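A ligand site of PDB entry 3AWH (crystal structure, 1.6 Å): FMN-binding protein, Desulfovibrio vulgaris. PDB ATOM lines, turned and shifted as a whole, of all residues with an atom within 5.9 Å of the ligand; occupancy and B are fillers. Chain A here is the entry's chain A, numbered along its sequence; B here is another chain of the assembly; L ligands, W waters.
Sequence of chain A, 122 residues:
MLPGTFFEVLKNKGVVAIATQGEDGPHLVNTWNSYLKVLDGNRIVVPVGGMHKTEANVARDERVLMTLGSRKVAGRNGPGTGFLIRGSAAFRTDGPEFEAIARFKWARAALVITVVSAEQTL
A ring nitrogen (NE2) of His 27 sits at hydrogen-bond distance from an oxygen (O7) of the ligand (2.7 Å).
An oxygen (O9) of the ligand lies within hydrogen-bond range of the backbone NH of Thr 54 (2.8 Å).
The side-chain hydroxyl of Thr 54 sits at hydrogen-bond distance from an oxygen (O9) of the ligand (2.7 Å).
The side-chain hydroxyl of Thr 31 lies within hydrogen-bond range of an oxygen (O2) of the ligand.
N of Gly 49 sits at hydrogen-bond distance from O1 of the ligand, 2.8 Å away.
An oxygen (O5) of the ligand is in hydrogen-bond range of the backbone NH of Met 51, 2.8 Å away.
An oxygen (O3) of the ligand is in hydrogen-bond range of the backbone NH (N) of Asn 30, at 2.8 Å.
The backbone carbonyl oxygen (O) of Asn 30 sits close to an oxygen (O3) of the ligand (3.4 Å).
N of Gly 50 is in hydrogen-bond range of O1 of the ligand.
An oxygen (O8) of the ligand sits at hydrogen-bond distance from the backbone NH of His 52.
The backbone carbonyl oxygen of Pro 47 is in hydrogen-bond range of a nitrogen (N2) of the ligand, 3.0 Å away.
N of Lys 53 is in hydrogen-bond range of O8 of the ligand, 3.1 Å away.
The backbone NH (N) of Thr 121 of chain B sits at hydrogen-bond distance from the backbone carbonyl oxygen (O) of Gly 82 of chain B (3.0 Å).
O of Leu 122 of chain B lies within hydrogen-bond range of OG1 of Thr 81 of chain B, at 2.7 Å.
CG2 of Val 15 touches C7 of the ligand, at 3.9 Å.
Val 29 touches the ligand.
Trp 32 touches the ligand (CZ2 to C7, 3.4 Å).
CD2 of Tyr 35 touches O2 of the ligand, 3.6 Å away.
C of Val 48 touches O1 of the ligand, 3.7 Å away.
CH2 of Trp 106 touches O2 of the ligand, at 3.6 Å.
Gly 82 of chain B touches the ligand (CA to C9, 3.4 Å).
Thr 121 of chain B touches the ligand.
Leu 122 of chain B touches the ligand (CD2 to C6, 3.9 Å).
Hydrophobic or aromatic side chains that line the ligand: Val 15, His 27, Val 29, Trp 32, Tyr 35, Met 51, His 52, Trp 106 and Leu 122 of chain B.
Water W1 lies within hydrogen-bond range of the side-chain amide oxygen of Asn 30 (2.7 Å), the side-chain hydroxyl of Thr 121 of chain B (2.7 Å) and an oxygen (O3) of the ligand (2.8 Å).
Water W3 lies within hydrogen-bond range of O4 of the ligand and O of Thr 121 of chain B.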
ATOM      1  N   VAL A  15      -1.741  12.458 -35.165  1.00  0.00           N
ATOM      2  CA  VAL A  15      -2.143  11.253 -34.459  1.00  0.00           C
ATOM      3  C   VAL A  15      -2.546  10.196 -35.468  1.00  0.00           C
ATOM      4  O   VAL A  15      -3.428  10.429 -36.315  1.00  0.00           O
ATOM      5  CB  VAL A  15      -3.315  11.567 -33.498  1.00  0.00           C
ATOM      6  CG1 VAL A  15      -3.850  10.302 -32.834  1.00  0.00           C
ATOM      7  CG2 VAL A  15      -2.904  12.588 -32.444  1.00  0.00           C
ATOM      8  N   HIS A  27     -11.085  -2.644 -31.623  1.00  0.00           N
ATOM      9  CA  HIS A  27     -10.248  -1.946 -30.665  1.00  0.00           C
ATOM     10  C   HIS A  27      -9.492  -0.877 -31.454  1.00  0.00           C
ATOM     11  O   HIS A  27      -9.230  -1.047 -32.639  1.00  0.00           O
ATOM     12  CB  HIS A  27      -9.291  -2.915 -29.963  1.00  0.00           C
ATOM     13  CG  HIS A  27      -8.598  -2.319 -28.772  1.00  0.00           C
ATOM     14  ND1 HIS A  27      -9.269  -1.959 -27.617  1.00  0.00           N
ATOM     15  CD2 HIS A  27      -7.293  -2.040 -28.544  1.00  0.00           C
ATOM     16  CE1 HIS A  27      -8.405  -1.476 -26.748  1.00  0.00           C
ATOM     17  NE2 HIS A  27      -7.202  -1.514 -27.284  1.00  0.00           N
ATOM     18  N   LEU A  28      -9.165   0.227 -30.783  1.00  0.00           N
ATOM     19  CA  LEU A  28      -8.584   1.370 -31.460  1.00  0.00           C
ATOM     20  C   LEU A  28      -7.509   1.998 -30.586  1.00  0.00           C
ATOM     21  O   LEU A  28      -7.761   2.372 -29.428  1.00  0.00           O
ATOM     22  CB  LEU A  28      -9.680   2.393 -31.800  1.00  0.00           C
ATOM     23  CG  LEU A  28      -9.291   3.656 -32.595  1.00  0.00           C
ATOM     24  CD1 LEU A  28      -8.749   3.250 -33.965  1.00  0.00           C
ATOM     25  CD2 LEU A  28     -10.478   4.605 -32.738  1.00  0.00           C
ATOM     26  N   VAL A  29      -6.300   2.089 -31.134  1.00  0.00           N
ATOM     27  CA  VAL A  29      -5.159   2.669 -30.439  1.00  0.00           C
ATOM     28  C   VAL A  29      -4.437   3.673 -31.338  1.00  0.00           C
ATOM     29  O   VAL A  29      -4.796   3.828 -32.513  1.00  0.00           O
ATOM     30  CB  VAL A  29      -4.162   1.599 -29.915  1.00  0.00           C
ATOM     31  CG1 VAL A  29      -4.874   0.636 -28.968  1.00  0.00           C
ATOM     32  CG2 VAL A  29      -3.508   0.838 -31.075  1.00  0.00           C
ATOM     33  N   ASN A  30      -3.424   4.331 -30.789  1.00  0.00           N
ATOM     34  CA  ASN A  30      -2.736   5.401 -31.505  1.00  0.00           C
ATOM     35  C   ASN A  30      -1.233   5.293 -31.520  1.00  0.00           C
ATOM     36  O   ASN A  30      -0.627   4.626 -30.689  1.00  0.00           O
ATOM     37  CB  ASN A  30      -3.093   6.748 -30.877  1.00  0.00           C
ATOM     38  CG  ASN A  30      -4.564   7.027 -30.914  1.00  0.00           C
ATOM     39  OD1 ASN A  30      -5.219   7.089 -29.872  1.00  0.00           O
ATOM     40  ND2 ASN A  30      -5.118   7.184 -32.116  1.00  0.00           N
ATOM     41  N   THR A  31      -0.631   5.987 -32.487  1.00  0.00           N
ATOM     42  CA  THR A  31       0.771   6.371 -32.408  1.00  0.00           C
ATOM     43  C   THR A  31       0.884   7.792 -32.990  1.00  0.00           C
ATOM     44  O   THR A  31      -0.131   8.472 -33.167  1.00  0.00           O
ATOM     45  CB  THR A  31       1.718   5.312 -33.036  1.00  0.00           C
ATOM     46  OG1 THR A  31       3.076   5.635 -32.735  1.00  0.00           O
ATOM     47  CG2 THR A  31       1.520   5.182 -34.539  1.00  0.00           C
ATOM     48  N   TRP A  32       2.100   8.253 -33.237  1.00  0.00           N
ATOM     49  CA  TRP A  32       2.319   9.569 -33.805  1.00  0.00           C
ATOM     50  C   TRP A  32       2.816   9.425 -35.246  1.00  0.00           C
ATOM     51  O   TRP A  32       3.512   8.449 -35.560  1.00  0.00           O
ATOM     52  CB  TRP A  32       3.377  10.302 -33.004  1.00  0.00           C
ATOM     53  CG  TRP A  32       3.022  10.622 -31.591  1.00  0.00           C
ATOM     54  CD1 TRP A  32       3.562  10.050 -30.454  1.00  0.00           C
ATOM     55  CD2 TRP A  32       2.095  11.611 -31.136  1.00  0.00           C
ATOM     56  NE1 TRP A  32       3.006  10.620 -29.334  1.00  0.00           N
ATOM     57  CE2 TRP A  32       2.112  11.580 -29.723  1.00  0.00           C
ATOM     58  CE3 TRP A  32       1.242  12.510 -31.788  1.00  0.00           C
ATOM     59  CZ2 TRP A  32       1.320  12.428 -28.944  1.00  0.00           C
ATOM     60  CZ3 TRP A  32       0.449  13.358 -31.008  1.00  0.00           C
ATOM     61  CH2 TRP A  32       0.483  13.308 -29.612  1.00  0.00           C
ATOM     62  N   TYR A  35       6.466   8.707 -35.690  1.00  0.00           N
ATOM     63  CA  TYR A  35       7.025   7.456 -35.177  1.00  0.00           C
ATOM     64  C   TYR A  35       7.003   6.340 -36.221  1.00  0.00           C
ATOM     65  O   TYR A  35       7.673   5.325 -36.039  1.00  0.00           O
ATOM     66  CB  TYR A  35       6.272   7.007 -33.908  1.00  0.00           C
ATOM     67  CG  TYR A  35       6.570   7.790 -32.644  1.00  0.00           C
ATOM     68  CD1 TYR A  35       7.296   8.984 -32.679  1.00  0.00           C
ATOM     69  CD2 TYR A  35       6.097   7.352 -31.420  1.00  0.00           C
ATOM     70  CE1 TYR A  35       7.564   9.712 -31.515  1.00  0.00           C
ATOM     71  CE2 TYR A  35       6.352   8.053 -30.256  1.00  0.00           C
ATOM     72  CZ  TYR A  35       7.086   9.232 -30.309  1.00  0.00           C
ATOM     73  OH  TYR A  35       7.326   9.928 -29.136  1.00  0.00           O
ATOM     74  N   VAL A  46       5.819   0.440 -36.340  1.00  0.00           N
ATOM     75  CA  VAL A  46       5.346   1.281 -35.234  1.00  0.00           C
ATOM     76  C   VAL A  46       6.035   0.820 -33.946  1.00  0.00           C
ATOM     77  O   VAL A  46       6.049  -0.382 -33.641  1.00  0.00           O
ATOM     78  CB  VAL A  46       3.814   1.131 -35.038  1.00  0.00           C
ATOM     79  CG1 VAL A  46       3.339   1.975 -33.851  1.00  0.00           C
ATOM     80  CG2 VAL A  46       3.040   1.533 -36.311  1.00  0.00           C
ATOM     81  N   PRO A  47       6.606   1.769 -33.168  1.00  0.00           N
ATOM     82  CA  PRO A  47       7.161   1.361 -31.872  1.00  0.00           C
ATOM     83  C   PRO A  47       6.054   1.037 -30.864  1.00  0.00           C
ATOM     84  O   PRO A  47       5.091   1.801 -30.737  1.00  0.00           O
ATOM     85  CB  PRO A  47       7.962   2.600 -31.445  1.00  0.00           C
ATOM     86  CG  PRO A  47       7.231   3.741 -32.092  1.00  0.00           C
ATOM     87  CD  PRO A  47       6.837   3.200 -33.442  1.00  0.00           C
ATOM     88  N   VAL A  48       6.193  -0.089 -30.174  1.00  0.00           N
ATOM     89  CA  VAL A  48       5.161  -0.572 -29.253  1.00  0.00           C
ATOM     90  C   VAL A  48       5.629  -0.482 -27.802  1.00  0.00           C
ATOM     91  O   VAL A  48       6.591  -1.153 -27.421  1.00  0.00           O
ATOM     92  CB  VAL A  48       4.767  -2.043 -29.555  1.00  0.00           C
ATOM     93  CG1 VAL A  48       3.776  -2.564 -28.523  1.00  0.00           C
ATOM     94  CG2 VAL A  48       4.155  -2.130 -30.944  1.00  0.00           C
ATOM     95  N   GLY A  49       4.954   0.355 -27.016  1.00  0.00           N
ATOM     96  CA  GLY A  49       5.166   0.421 -25.566  1.00  0.00           C
ATOM     97  C   GLY A  49       4.108  -0.421 -24.869  1.00  0.00           C
ATOM     98  O   GLY A  49       4.435  -1.324 -24.094  1.00  0.00           O
ATOM     99  N   GLY A  50       2.844  -0.124 -25.154  1.00  0.00           N
ATOM    100  CA  GLY A  50       1.710  -0.869 -24.597  1.00  0.00           C
ATOM    101  C   GLY A  50       1.171  -1.841 -25.622  1.00  0.00           C
ATOM    102  O   GLY A  50       1.763  -2.899 -25.871  1.00  0.00           O
ATOM    103  N   MET A  51       0.047  -1.465 -26.240  1.00  0.00           N
ATOM    104  CA  MET A  51      -0.628  -2.274 -27.268  1.00  0.00           C
ATOM    105  C   MET A  51      -0.769  -3.744 -26.908  1.00  0.00           C
ATOM    106  O   MET A  51      -0.528  -4.622 -27.737  1.00  0.00           O
ATOM    107  CB  MET A  51       0.057  -2.106 -28.631  1.00  0.00           C
ATOM    108  CG  MET A  51       0.074  -0.659 -29.107  1.00  0.00           C
ATOM    109  SD  MET A  51       0.434  -0.516 -30.855  1.00  0.00           S
ATOM    110  CE  MET A  51       0.662   1.251 -30.988  1.00  0.00           C
ATOM    111  N   HIS A  52      -1.158  -4.021 -25.667  1.00  0.00           N
ATOM    112  CA  HIS A  52      -1.342  -5.413 -25.239  1.00  0.00           C
ATOM    113  C   HIS A  52      -2.629  -6.009 -25.779  1.00  0.00           C
ATOM    114  O   HIS A  52      -2.633  -7.159 -26.251  1.00  0.00           O
ATOM    115  CB  HIS A  52      -1.292  -5.500 -23.715  1.00  0.00           C
ATOM    116  CG  HIS A  52       0.060  -5.211 -23.148  1.00  0.00           C
ATOM    117  ND1 HIS A  52       1.105  -6.101 -23.252  1.00  0.00           N
ATOM    118  CD2 HIS A  52       0.550  -4.129 -22.515  1.00  0.00           C
ATOM    119  CE1 HIS A  52       2.182  -5.583 -22.682  1.00  0.00           C
ATOM    120  NE2 HIS A  52       1.866  -4.383 -22.226  1.00  0.00           N
ATOM    121  N   LYS A  53      -3.712  -5.245 -25.730  1.00  0.00           N
ATOM    122  CA  LYS A  53      -4.978  -5.708 -26.290  1.00  0.00           C
ATOM    123  C   LYS A  53      -4.850  -5.792 -27.815  1.00  0.00           C
ATOM    124  O   LYS A  53      -5.296  -6.761 -28.412  1.00  0.00           O
ATOM    125  CB  LYS A  53      -6.132  -4.780 -25.910  1.00  0.00           C
ATOM    126  CG  LYS A  53      -6.428  -4.762 -24.421  1.00  0.00           C
ATOM    127  CD  LYS A  53      -7.818  -4.191 -24.151  1.00  0.00           C
ATOM    128  CE  LYS A  53      -7.993  -3.689 -22.711  1.00  0.00           C
ATOM    129  NZ  LYS A  53      -7.114  -4.380 -21.721  1.00  0.00           N
ATOM    130  N   THR A  54      -4.221  -4.779 -28.413  1.00  0.00           N
ATOM    131  CA  THR A  54      -3.939  -4.755 -29.836  1.00  0.00           C
ATOM    132  C   THR A  54      -3.136  -5.985 -30.285  1.00  0.00           C
ATOM    133  O   THR A  54      -3.452  -6.575 -31.316  1.00  0.00           O
ATOM    134  CB  THR A  54      -3.220  -3.447 -30.226  1.00  0.00           C
ATOM    135  OG1 THR A  54      -4.085  -2.359 -29.925  1.00  0.00           O
ATOM    136  CG2 THR A  54      -2.851  -3.400 -31.701  1.00  0.00           C
ATOM    137  N   GLU A  55      -2.137  -6.374 -29.499  1.00  0.00           N
ATOM    138  CA  GLU A  55      -1.305  -7.525 -29.840  1.00  0.00           C
ATOM    139  C   GLU A  55      -2.123  -8.808 -29.769  1.00  0.00           C
ATOM    140  O   GLU A  55      -2.003  -9.654 -30.658  1.00  0.00           O
ATOM    141  CB  GLU A  55      -0.087  -7.637 -28.930  1.00  0.00           C
ATOM    142  CG  GLU A  55       0.877  -8.732 -29.370  1.00  0.00           C
ATOM    143  CD  GLU A  55       2.113  -8.865 -28.496  1.00  0.00           C
ATOM    144  OE1 GLU A  55       2.243  -8.133 -27.493  1.00  0.00           O
ATOM    145  OE2 GLU A  55       2.947  -9.741 -28.821  1.00  0.00           O
ATOM    146  N   TRP A 106      11.708   2.845 -24.906  1.00  0.00           N
ATOM    147  CA  TRP A 106      10.512   2.342 -24.247  1.00  0.00           C
ATOM    148  C   TRP A 106       9.799   1.249 -25.041  1.00  0.00           C
ATOM    149  O   TRP A 106       8.830   0.669 -24.548  1.00  0.00           O
ATOM    150  CB  TRP A 106       9.532   3.496 -23.946  1.00  0.00           C
ATOM    151  CG  TRP A 106       9.310   4.426 -25.125  1.00  0.00           C
ATOM    152  CD1 TRP A 106       9.956   5.607 -25.371  1.00  0.00           C
ATOM    153  CD2 TRP A 106       8.383   4.230 -26.212  1.00  0.00           C
ATOM    154  NE1 TRP A 106       9.487   6.155 -26.537  1.00  0.00           N
ATOM    155  CE2 TRP A 106       8.524   5.342 -27.076  1.00  0.00           C
ATOM    156  CE3 TRP A 106       7.452   3.231 -26.536  1.00  0.00           C
ATOM    157  CZ2 TRP A 106       7.769   5.484 -28.252  1.00  0.00           C
ATOM    158  CZ3 TRP A 106       6.695   3.374 -27.703  1.00  0.00           C
ATOM    159  CH2 TRP A 106       6.859   4.498 -28.534  1.00  0.00           C
ATOM    160  N   LEU B  68      -8.415  10.831 -30.528  1.00  0.00           N
ATOM    161  CA  LEU B  68      -7.972  12.157 -30.956  1.00  0.00           C
ATOM    162  C   LEU B  68      -6.856  12.580 -30.027  1.00  0.00           C
ATOM    163  O   LEU B  68      -6.733  12.059 -28.920  1.00  0.00           O
ATOM    164  CB  LEU B  68      -9.116  13.170 -30.917  1.00  0.00           C
ATOM    165  CG  LEU B  68      -9.689  13.601 -29.564  1.00  0.00           C
ATOM    166  CD1 LEU B  68     -10.435  14.906 -29.752  1.00  0.00           C
ATOM    167  CD2 LEU B  68     -10.595  12.531 -28.937  1.00  0.00           C
ATOM    168  N   GLY B  69      -6.035  13.529 -30.483  1.00  0.00           N
ATOM    169  CA  GLY B  69      -4.932  13.988 -29.640  1.00  0.00           C
ATOM    170  C   GLY B  69      -4.192  15.182 -30.199  1.00  0.00           C
ATOM    171  O   GLY B  69      -4.577  15.751 -31.214  1.00  0.00           O
ATOM    172  N   SER B  70      -3.114  15.548 -29.524  1.00  0.00           N
ATOM    173  CA  SER B  70      -2.307  16.692 -29.958  1.00  0.00           C
ATOM    174  C   SER B  70      -0.917  16.645 -29.355  1.00  0.00           C
ATOM    175  O   SER B  70      -0.780  16.407 -28.150  1.00  0.00           O
ATOM    176  CB  SER B  70      -2.985  18.005 -29.561  1.00  0.00           C
ATOM    177  OG  SER B  70      -2.163  19.111 -29.929  1.00  0.00           O
ATOM    178  N   THR B  81      -0.544  14.344 -25.903  1.00  0.00           N
ATOM    179  CA  THR B  81      -1.572  13.564 -25.217  1.00  0.00           C
ATOM    180  C   THR B  81      -2.679  13.170 -26.188  1.00  0.00           C
ATOM    181  O   THR B  81      -2.699  13.608 -27.335  1.00  0.00           O
ATOM    182  CB  THR B  81      -2.166  14.332 -23.999  1.00  0.00           C
ATOM    183  OG1 THR B  81      -2.909  13.424 -23.173  1.00  0.00           O
ATOM    184  CG2 THR B  81      -3.093  15.438 -24.446  1.00  0.00           C
ATOM    185  N   GLY B  82      -3.593  12.342 -25.705  1.00  0.00           N
ATOM    186  CA  GLY B  82      -4.771  12.009 -26.489  1.00  0.00           C
ATOM    187  C   GLY B  82      -5.743  11.174 -25.689  1.00  0.00           C
ATOM    188  O   GLY B  82      -5.484  10.823 -24.529  1.00  0.00           O
ATOM    189  N   PHE B  83      -6.873  10.855 -26.326  1.00  0.00           N
ATOM    190  CA  PHE B  83      -7.994  10.208 -25.654  1.00  0.00           C
ATOM    191  C   PHE B  83      -8.576   9.097 -26.479  1.00  0.00           C
ATOM    192  O   PHE B  83      -8.613   9.176 -27.717  1.00  0.00           O
ATOM    193  CB  PHE B  83      -9.111  11.216 -25.337  1.00  0.00           C
ATOM    194  CG  PHE B  83      -8.743  12.213 -24.287  1.00  0.00           C
ATOM    195  CD1 PHE B  83      -8.040  13.365 -24.615  1.00  0.00           C
ATOM    196  CD2 PHE B  83      -9.101  11.990 -22.956  1.00  0.00           C
ATOM    197  CE1 PHE B  83      -7.678  14.275 -23.638  1.00  0.00           C
ATOM    198  CE2 PHE B  83      -8.750  12.906 -21.961  1.00  0.00           C
ATOM    199  CZ  PHE B  83      -8.042  14.044 -22.297  1.00  0.00           C
ATOM    200  N   THR B 121      -5.065   8.449 -22.745  1.00  0.00           N
ATOM    201  CA  THR B 121      -4.232   7.267 -22.982  1.00  0.00           C
ATOM    202  C   THR B 121      -2.753   7.586 -23.130  1.00  0.00           C
ATOM    203  O   THR B 121      -1.941   6.699 -23.427  1.00  0.00           O
ATOM    204  CB  THR B 121      -4.719   6.496 -24.221  1.00  0.00           C
ATOM    205  OG1 THR B 121      -4.952   7.424 -25.279  1.00  0.00           O
ATOM    206  CG2 THR B 121      -6.018   5.733 -23.917  1.00  0.00           C
ATOM    207  N   LEU B 122      -2.413   8.858 -22.919  1.00  0.00           N
ATOM    208  CA  LEU B 122      -1.019   9.310 -22.928  1.00  0.00           C
ATOM    209  C   LEU B 122      -0.846  10.494 -21.992  1.00  0.00           C
ATOM    210  O   LEU B 122      -1.730  11.342 -21.903  1.00  0.00           O
ATOM    211  CB  LEU B 122      -0.594   9.663 -24.363  1.00  0.00           C
ATOM    212  CG  LEU B 122       0.866  10.021 -24.619  1.00  0.00           C
ATOM    213  CD1 LEU B 122       1.772   8.805 -24.468  1.00  0.00           C
ATOM    214  CD2 LEU B 122       1.027  10.610 -26.019  1.00  0.00           C
ATOM    215  OXT LEU B 122       0.169  10.636 -21.294  1.00  0.00           O
HETATM  216  N1  LIG L   1       1.246   3.294 -27.443  1.00  0.00           N
HETATM  217  C1  LIG L   1       2.298   2.586 -27.998  1.00  0.00           C
HETATM  218  O1  LIG L   1       2.507   1.426 -27.671  1.00  0.00           O
HETATM  219  N2  LIG L   1       3.142   3.190 -28.925  1.00  0.00           N
HETATM  220  C2  LIG L   1       2.950   4.505 -29.325  1.00  0.00           C
HETATM  221  O2  LIG L   1       3.730   4.987 -30.147  1.00  0.00           O
HETATM  222  C3  LIG L   1       1.893   5.227 -28.771  1.00  0.00           C
HETATM  223  N3  LIG L   1       1.680   6.552 -29.144  1.00  0.00           N
HETATM  224  C4  LIG L   1       0.504   7.193 -28.761  1.00  0.00           C
HETATM  225  C5  LIG L   1       0.206   8.431 -29.330  1.00  0.00           C
HETATM  226  C6  LIG L   1      -0.974   9.083 -28.959  1.00  0.00           C
HETATM  227  C7  LIG L   1      -1.324  10.432 -29.575  1.00  0.00           C
HETATM  228  C8  LIG L   1      -1.837   8.511 -28.027  1.00  0.00           C
HETATM  229  C9  LIG L   1      -3.128   9.227 -27.615  1.00  0.00           C
HETATM  230  C10 LIG L   1      -1.534   7.281 -27.468  1.00  0.00           C
HETATM  231  C11 LIG L   1      -0.361   6.621 -27.820  1.00  0.00           C
HETATM  232  N4  LIG L   1      -0.053   5.344 -27.287  1.00  0.00           N
HETATM  233  C12 LIG L   1       1.044   4.637 -27.836  1.00  0.00           C
HETATM  234  C13 LIG L   1      -0.986   4.626 -26.402  1.00  0.00           C
HETATM  235  C14 LIG L   1      -1.834   3.639 -27.233  1.00  0.00           C
HETATM  236  O3  LIG L   1      -2.773   4.385 -28.054  1.00  0.00           O
HETATM  237  C15 LIG L   1      -2.606   2.635 -26.371  1.00  0.00           C
HETATM  238  O4  LIG L   1      -3.503   3.358 -25.513  1.00  0.00           O
HETATM  239  C16 LIG L   1      -1.687   1.711 -25.516  1.00  0.00           C
HETATM  240  O5  LIG L   1      -0.556   1.269 -26.268  1.00  0.00           O
HETATM  241  C17 LIG L   1      -2.451   0.506 -24.979  1.00  0.00           C
HETATM  242  O6  LIG L   1      -2.851  -0.312 -26.071  1.00  0.00           O
HETATM  243  P1  LIG L   1      -3.913  -1.511 -25.918  1.00  0.00           P
HETATM  244  O7  LIG L   1      -5.270  -0.819 -25.513  1.00  0.00           O
HETATM  245  O8  LIG L   1      -3.417  -2.346 -24.651  1.00  0.00           O
HETATM  246  O9  LIG L   1      -3.970  -2.264 -27.204  1.00  0.00           O
HETATM  247  O   HOH W   1      -5.079   5.793 -27.475  1.00  0.00           O
HETATM  248  O   HOH W   2       1.112   2.965 -23.976  1.00  0.00           O
HETATM  249  O   HOH W   3      -2.747   3.912 -22.881  1.00  0.00           O
HETATM  250  O   HOH W   4      -3.171  -1.833 -22.144  1.00  0.00           O
HETATM  251  O   HOH W   5      -6.436  -0.906 -23.096  1.00  0.00           O
HETATM  252  O   HOH W   6      -5.815   1.818 -25.302  1.00  0.00           O
